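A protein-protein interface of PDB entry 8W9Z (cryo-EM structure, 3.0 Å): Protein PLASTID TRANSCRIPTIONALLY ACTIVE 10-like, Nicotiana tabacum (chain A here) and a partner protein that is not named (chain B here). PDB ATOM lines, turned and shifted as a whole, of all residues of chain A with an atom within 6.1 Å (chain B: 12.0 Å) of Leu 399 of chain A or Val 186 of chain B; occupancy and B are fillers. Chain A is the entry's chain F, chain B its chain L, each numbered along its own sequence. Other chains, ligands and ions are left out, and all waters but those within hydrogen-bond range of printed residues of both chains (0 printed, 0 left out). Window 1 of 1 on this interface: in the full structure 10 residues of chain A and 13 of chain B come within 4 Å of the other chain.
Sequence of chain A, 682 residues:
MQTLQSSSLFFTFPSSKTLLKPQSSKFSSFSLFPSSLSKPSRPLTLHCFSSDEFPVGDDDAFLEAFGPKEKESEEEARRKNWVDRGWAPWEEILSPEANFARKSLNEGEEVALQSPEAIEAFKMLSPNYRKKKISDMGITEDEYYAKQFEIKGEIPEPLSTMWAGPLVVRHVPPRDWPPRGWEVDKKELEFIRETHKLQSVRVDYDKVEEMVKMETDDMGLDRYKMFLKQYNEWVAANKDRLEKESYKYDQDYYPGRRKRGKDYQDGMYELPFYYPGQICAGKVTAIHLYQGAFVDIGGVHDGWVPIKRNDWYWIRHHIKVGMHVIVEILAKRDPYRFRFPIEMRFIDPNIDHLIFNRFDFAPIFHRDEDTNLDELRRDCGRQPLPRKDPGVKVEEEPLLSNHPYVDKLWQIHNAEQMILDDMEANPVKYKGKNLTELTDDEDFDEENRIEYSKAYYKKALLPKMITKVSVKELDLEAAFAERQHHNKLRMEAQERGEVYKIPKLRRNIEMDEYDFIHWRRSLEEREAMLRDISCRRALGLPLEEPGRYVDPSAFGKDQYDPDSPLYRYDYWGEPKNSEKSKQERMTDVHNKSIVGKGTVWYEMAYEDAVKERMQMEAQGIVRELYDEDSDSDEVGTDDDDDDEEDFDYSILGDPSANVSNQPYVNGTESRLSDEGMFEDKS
Printed residues of chain B that touch a printed residue of chain A: Val 186, Gly 187, Asn 188, Thr 189, Ser 190 and Asn 191. Hydrophobic or aromatic side chains of chain A that line the printed part of chain B: Pro 398, Leu 399 and Trp 519. Among the printed residues, 8 pairs touch across the chains. Among the printed residues, no Asp or Glu carboxylate lies within 4 Å of a Lys or Arg side-chain nitrogen of the other chain.
Glu 397 of chain A touches Val 186 of chain B. CA of Gly 187 of chain B touches CB of Pro 398 of chain A (3.8 Å). Val 186 of chain B touches Leu 399 of chain A. Thr 189 of chain B touches Trp 519 of chain A (O to CZ2, 3.1 Å). CZ2 of Trp 519 of chain A touches O of Ser 190 of chain B, at 3.3 Å. Asn 191 of chain B touches Trp 519 of chain A (CG to CH2, 3.4 Å).
ND2 of Asn 188 of chain B sits at hydrogen-bond distance from OG of Ser 401 of chain A (3.0 Å). The backbone carbonyl oxygen of Asn 188 of chain B lies within hydrogen-bond range of the indole nitrogen of Trp 519 of chain A, 2.5 Å away.
OD1 of Asn 191 of chain B sits close to O of Thr 189 of chain B. NH2 of Arg 526 of chain A is in salt-bridge range of OE2 of Glu 397 of chain A, 3.4 Å away. O of Pro 398 of chain A is in hydrogen-bond range of NH2 of Arg 526 of chain A (2.9 Å).
Printed residues of chain B within 4 Å of Leu 399 of chain A: Val 186 (3.4 Å). Val 186 of chain B touches two residues of chain A. No residue of chain B comes within 4 Å of Glu 395 of chain A. Of the printed residues of chain B, Glu 397 of chain A touches Val 186. Pro 398 of chain A touches just one residue of chain B: Gly 187. No residue of chain B comes within 4 Å of Leu 400 of chain A. Ser 401 of chain A touches one residue of chain B. Of chain B, only Asn 188 (2.5 Å), Thr 189 (3.1 Å), Ser 190 (3.3 Å) and Asn 191 (3.4 Å) come within 4 Å of Trp 519 of chain A. Ser 522 of chain A touches none of the printed residues of chain B. Of the printed residues of chain A, Ser 190 of chain B touches Trp 519 (3.3 Å). Printed residues of chain A within 4 Å of Asn 188 of chain B: Ser 401 and Trp 519. Printed residues of chain A within 4 Å of Thr 189 of chain B: Trp 519. Of the printed residues of chain A, Asn 191 of chain B touches Trp 519. The nearest residue of chain B that does not touch Leu 399 of chain A is Asn 188 of chain B (4.1 Å). The nearest residue of chain A that does not touch Val 186 of chain B is Glu 395 of chain A (4.1 Å).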
ATOM      1  N   GLU A 395       5.974  13.168  24.058  1.00  0.00           N
ATOM      2  CA  GLU A 395       6.281  13.992  22.895  1.00  0.00           C
ATOM      3  C   GLU A 395       5.495  13.566  21.661  1.00  0.00           C
ATOM      4  O   GLU A 395       5.149  14.414  20.831  1.00  0.00           O
ATOM      5  CB  GLU A 395       7.781  13.947  22.599  1.00  0.00           C
ATOM      6  N   GLU A 396       5.207  12.273  21.521  1.00  0.00           N
ATOM      7  CA  GLU A 396       4.498  11.758  20.348  1.00  0.00           C
ATOM      8  C   GLU A 396       3.003  11.655  20.652  1.00  0.00           C
ATOM      9  O   GLU A 396       2.413  10.576  20.727  1.00  0.00           O
ATOM     10  CB  GLU A 396       5.080  10.414  19.926  1.00  0.00           C
ATOM     11  N   GLU A 397       2.387  12.824  20.823  1.00  0.00           N
ATOM     12  CA  GLU A 397       0.961  12.913  21.099  1.00  0.00           C
ATOM     13  C   GLU A 397       0.476  14.293  20.687  1.00  0.00           C
ATOM     14  O   GLU A 397       1.254  15.253  20.727  1.00  0.00           O
ATOM     15  CB  GLU A 397       0.664  12.656  22.583  1.00  0.00           C
ATOM     16  CG  GLU A 397       1.429  13.551  23.540  1.00  0.00           C
ATOM     17  CD  GLU A 397       1.066  13.298  24.989  1.00  0.00           C
ATOM     18  OE1 GLU A 397       0.206  12.428  25.245  1.00  0.00           O
ATOM     19  OE2 GLU A 397       1.639  13.968  25.874  1.00  0.00           O
ATOM     20  N   PRO A 398      -0.784  14.427  20.283  1.00  0.00           N
ATOM     21  CA  PRO A 398      -1.280  15.730  19.828  1.00  0.00           C
ATOM     22  C   PRO A 398      -1.391  16.727  20.971  1.00  0.00           C
ATOM     23  O   PRO A 398      -1.337  16.380  22.153  1.00  0.00           O
ATOM     24  CB  PRO A 398      -2.658  15.403  19.245  1.00  0.00           C
ATOM     25  CG  PRO A 398      -3.077  14.164  19.960  1.00  0.00           C
ATOM     26  CD  PRO A 398      -1.815  13.379  20.177  1.00  0.00           C
ATOM     27  N   LEU A 399      -1.550  17.993  20.591  1.00  0.00           N
ATOM     28  CA  LEU A 399      -1.659  19.079  21.551  1.00  0.00           C
ATOM     29  C   LEU A 399      -3.090  19.183  22.076  1.00  0.00           C
ATOM     30  O   LEU A 399      -3.965  18.376  21.750  1.00  0.00           O
ATOM     31  CB  LEU A 399      -1.209  20.395  20.919  1.00  0.00           C
ATOM     32  CG  LEU A 399       0.292  20.654  20.753  1.00  0.00           C
ATOM     33  CD1 LEU A 399       0.910  19.783  19.668  1.00  0.00           C
ATOM     34  CD2 LEU A 399       0.542  22.128  20.465  1.00  0.00           C
ATOM     35  N   LEU A 400      -3.330  20.197  22.901  1.00  0.00           N
ATOM     36  CA  LEU A 400      -4.635  20.446  23.498  1.00  0.00           C
ATOM     37  C   LEU A 400      -5.167  21.779  22.990  1.00  0.00           C
ATOM     38  O   LEU A 400      -4.470  22.796  23.060  1.00  0.00           O
ATOM     39  CB  LEU A 400      -4.541  20.450  25.027  1.00  0.00           C
ATOM     40  CG  LEU A 400      -5.761  20.007  25.842  1.00  0.00           C
ATOM     41  CD1 LEU A 400      -5.348  19.696  27.270  1.00  0.00           C
ATOM     42  CD2 LEU A 400      -6.856  21.060  25.827  1.00  0.00           C
ATOM     43  N   SER A 401      -6.396  21.769  22.481  1.00  0.00           N
ATOM     44  CA  SER A 401      -7.020  22.963  21.917  1.00  0.00           C
ATOM     45  C   SER A 401      -8.454  23.095  22.420  1.00  0.00           C
ATOM     46  O   SER A 401      -9.388  23.345  21.657  1.00  0.00           O
ATOM     47  CB  SER A 401      -6.974  22.929  20.390  1.00  0.00           C
ATOM     48  OG  SER A 401      -5.639  22.853  19.923  1.00  0.00           O
ATOM     49  N   TRP A 519      -4.083  27.085  22.814  1.00  0.00           N
ATOM     50  CA  TRP A 519      -3.238  26.335  21.891  1.00  0.00           C
ATOM     51  C   TRP A 519      -1.813  26.869  21.899  1.00  0.00           C
ATOM     52  O   TRP A 519      -0.853  26.095  21.817  1.00  0.00           O
ATOM     53  CB  TRP A 519      -3.825  26.389  20.482  1.00  0.00           C
ATOM     54  CG  TRP A 519      -2.978  25.703  19.457  1.00  0.00           C
ATOM     55  CD1 TRP A 519      -3.073  24.405  19.052  1.00  0.00           C
ATOM     56  CD2 TRP A 519      -1.903  26.280  18.707  1.00  0.00           C
ATOM     57  NE1 TRP A 519      -2.124  24.137  18.096  1.00  0.00           N
ATOM     58  CE2 TRP A 519      -1.393  25.272  17.867  1.00  0.00           C
ATOM     59  CE3 TRP A 519      -1.322  27.551  18.666  1.00  0.00           C
ATOM     60  CZ2 TRP A 519      -0.332  25.495  16.995  1.00  0.00           C
ATOM     61  CZ3 TRP A 519      -0.269  27.770  17.800  1.00  0.00           C
ATOM     62  CH2 TRP A 519       0.216  26.748  16.976  1.00  0.00           C
ATOM     63  N   SER A 522      -0.118  25.545  25.015  1.00  0.00           N
ATOM     64  CA  SER A 522       0.289  24.153  24.835  1.00  0.00           C
ATOM     65  C   SER A 522       1.491  24.041  23.902  1.00  0.00           C
ATOM     66  O   SER A 522       2.393  23.220  24.127  1.00  0.00           O
ATOM     67  CB  SER A 522      -0.881  23.328  24.302  1.00  0.00           C
ATOM     68  OG  SER A 522      -0.498  21.981  24.094  1.00  0.00           O
ATOM     69  N   LEU A 523       1.520  24.859  22.847  1.00  0.00           N
ATOM     70  CA  LEU A 523       2.649  24.845  21.924  1.00  0.00           C
ATOM     71  C   LEU A 523       3.934  25.269  22.620  1.00  0.00           C
ATOM     72  O   LEU A 523       4.988  24.659  22.413  1.00  0.00           O
ATOM     73  CB  LEU A 523       2.365  25.758  20.732  1.00  0.00           C
ATOM     74  CG  LEU A 523       3.525  25.940  19.750  1.00  0.00           C
ATOM     75  CD1 LEU A 523       3.818  24.642  19.013  1.00  0.00           C
ATOM     76  CD2 LEU A 523       3.241  27.069  18.772  1.00  0.00           C
ATOM     77  N   ARG A 526       5.125  22.370  24.871  1.00  0.00           N
ATOM     78  CA  ARG A 526       5.801  21.283  24.165  1.00  0.00           C
ATOM     79  C   ARG A 526       7.117  21.738  23.548  1.00  0.00           C
ATOM     80  O   ARG A 526       8.057  20.941  23.442  1.00  0.00           O
ATOM     81  CB  ARG A 526       4.885  20.678  23.104  1.00  0.00           C
ATOM     82  CG  ARG A 526       4.176  19.426  23.587  1.00  0.00           C
ATOM     83  CD  ARG A 526       3.341  18.783  22.500  1.00  0.00           C
ATOM     84  NE  ARG A 526       2.564  17.663  23.019  1.00  0.00           N
ATOM     85  CZ  ARG A 526       1.390  17.790  23.627  1.00  0.00           C
ATOM     86  NH1 ARG A 526       0.856  18.992  23.796  1.00  0.00           N
ATOM     87  NH2 ARG A 526       0.748  16.719  24.071  1.00  0.00           N
ATOM     88  N   ASN B 182      10.740  26.928  13.794  1.00  0.00           N
ATOM     89  CA  ASN B 182      10.498  25.504  13.944  1.00  0.00           C
ATOM     90  C   ASN B 182       9.058  25.152  13.578  1.00  0.00           C
ATOM     91  O   ASN B 182       8.193  26.016  13.426  1.00  0.00           O
ATOM     92  CB  ASN B 182      10.804  25.059  15.374  1.00  0.00           C
ATOM     93  N   ARG B 183       8.813  23.852  13.439  1.00  0.00           N
ATOM     94  CA  ARG B 183       7.483  23.340  13.127  1.00  0.00           C
ATOM     95  C   ARG B 183       7.376  21.935  13.695  1.00  0.00           C
ATOM     96  O   ARG B 183       8.199  21.073  13.373  1.00  0.00           O
ATOM     97  CB  ARG B 183       7.229  23.337  11.619  1.00  0.00           C
ATOM     98  N   LEU B 184       6.370  21.707  14.536  1.00  0.00           N
ATOM     99  CA  LEU B 184       6.204  20.411  15.173  1.00  0.00           C
ATOM    100  C   LEU B 184       5.810  19.353  14.144  1.00  0.00           C
ATOM    101  O   LEU B 184       5.549  19.644  12.972  1.00  0.00           O
ATOM    102  CB  LEU B 184       5.155  20.493  16.282  1.00  0.00           C
ATOM    103  N   ASN B 185       5.769  18.102  14.601  1.00  0.00           N
ATOM    104  CA  ASN B 185       5.419  16.971  13.750  1.00  0.00           C
ATOM    105  C   ASN B 185       4.421  16.051  14.442  1.00  0.00           C
ATOM    106  O   ASN B 185       4.394  14.846  14.180  1.00  0.00           O
ATOM    107  CB  ASN B 185       6.666  16.192  13.336  1.00  0.00           C
ATOM    108  N   VAL B 186       3.596  16.602  15.330  1.00  0.00           N
ATOM    109  CA  VAL B 186       2.613  15.809  16.055  1.00  0.00           C
ATOM    110  C   VAL B 186       1.391  16.662  16.368  1.00  0.00           C
ATOM    111  O   VAL B 186       1.501  17.715  17.006  1.00  0.00           O
ATOM    112  CB  VAL B 186       3.214  15.219  17.344  1.00  0.00           C
ATOM    113  N   GLY B 187       0.230  16.296  15.883  1.00  0.00           N
ATOM    114  CA  GLY B 187      -0.967  17.003  16.261  1.00  0.00           C
ATOM    115  C   GLY B 187      -1.253  18.327  15.665  1.00  0.00           C
ATOM    116  O   GLY B 187      -0.948  18.566  14.507  1.00  0.00           O
ATOM    117  N   ASN B 188      -1.816  19.219  16.461  1.00  0.00           N
ATOM    118  CA  ASN B 188      -2.201  20.501  15.979  1.00  0.00           C
ATOM    119  C   ASN B 188      -1.020  21.415  15.952  1.00  0.00           C
ATOM    120  O   ASN B 188      -1.023  22.423  16.609  1.00  0.00           O
ATOM    121  CB  ASN B 188      -3.200  21.081  16.949  1.00  0.00           C
ATOM    122  CG  ASN B 188      -4.328  20.133  17.267  1.00  0.00           C
ATOM    123  OD1 ASN B 188      -4.547  19.148  16.567  1.00  0.00           O
ATOM    124  ND2 ASN B 188      -5.061  20.434  18.327  1.00  0.00           N
ATOM    125  N   THR B 189       0.007  21.092  15.208  1.00  0.00           N
ATOM    126  CA  THR B 189       1.146  21.971  15.079  1.00  0.00           C
ATOM    127  C   THR B 189       0.890  23.272  14.348  1.00  0.00           C
ATOM    128  O   THR B 189       1.447  24.296  14.727  1.00  0.00           O
ATOM    129  CB  THR B 189       2.285  21.253  14.357  1.00  0.00           C
ATOM    130  N   SER B 190       0.093  23.255  13.281  1.00  0.00           N
ATOM    131  CA  SER B 190      -0.112  24.460  12.474  1.00  0.00           C
ATOM    132  C   SER B 190      -0.775  25.623  13.193  1.00  0.00           C
ATOM    133  O   SER B 190      -1.678  25.425  13.990  1.00  0.00           O
ATOM    134  CB  SER B 190      -0.909  24.113  11.221  1.00  0.00           C
ATOM    135  N   ASN B 191      -0.364  26.844  12.891  1.00  0.00           N
ATOM    136  CA  ASN B 191      -0.871  27.993  13.615  1.00  0.00           C
ATOM    137  C   ASN B 191      -1.994  28.622  12.938  1.00  0.00           C
ATOM    138  O   ASN B 191      -1.927  28.926  11.751  1.00  0.00           O
ATOM    139  CB  ASN B 191       0.186  29.094  13.708  1.00  0.00           C
ATOM    140  CG  ASN B 191       1.418  28.669  14.481  1.00  0.00           C
ATOM    141  OD1 ASN B 191       2.019  27.631  14.203  1.00  0.00           O
ATOM    142  ND2 ASN B 191       1.808  29.483  15.455  1.00  0.00           N
ATOM    143  N   PRO B 192      -3.063  28.840  13.674  1.00  0.00           N
ATOM    144  CA  PRO B 192      -4.100  29.609  13.040  1.00  0.00           C
ATOM    145  C   PRO B 192      -3.570  31.000  13.158  1.00  0.00           C
ATOM    146  O   PRO B 192      -2.681  31.219  13.971  1.00  0.00           O
ATOM    147  CB  PRO B 192      -5.244  29.413  13.984  1.00  0.00           C
ATOM    148  N   ASP B 216      15.614  21.987  15.495  1.00  0.00           N
ATOM    149  CA  ASP B 216      15.276  22.769  14.300  1.00  0.00           C
ATOM    150  C   ASP B 216      15.216  24.262  14.434  1.00  0.00           C
ATOM    151  O   ASP B 216      14.425  24.913  13.767  1.00  0.00           O
ATOM    152  CB  ASP B 216      13.984  22.262  13.669  1.00  0.00           C
ATOM    153  CG  ASP B 216      14.075  20.822  13.242  1.00  0.00           C
ATOM    154  OD1 ASP B 216      15.204  20.304  13.136  1.00  0.00           O
ATOM    155  OD2 ASP B 216      13.016  20.207  13.005  1.00  0.00           O
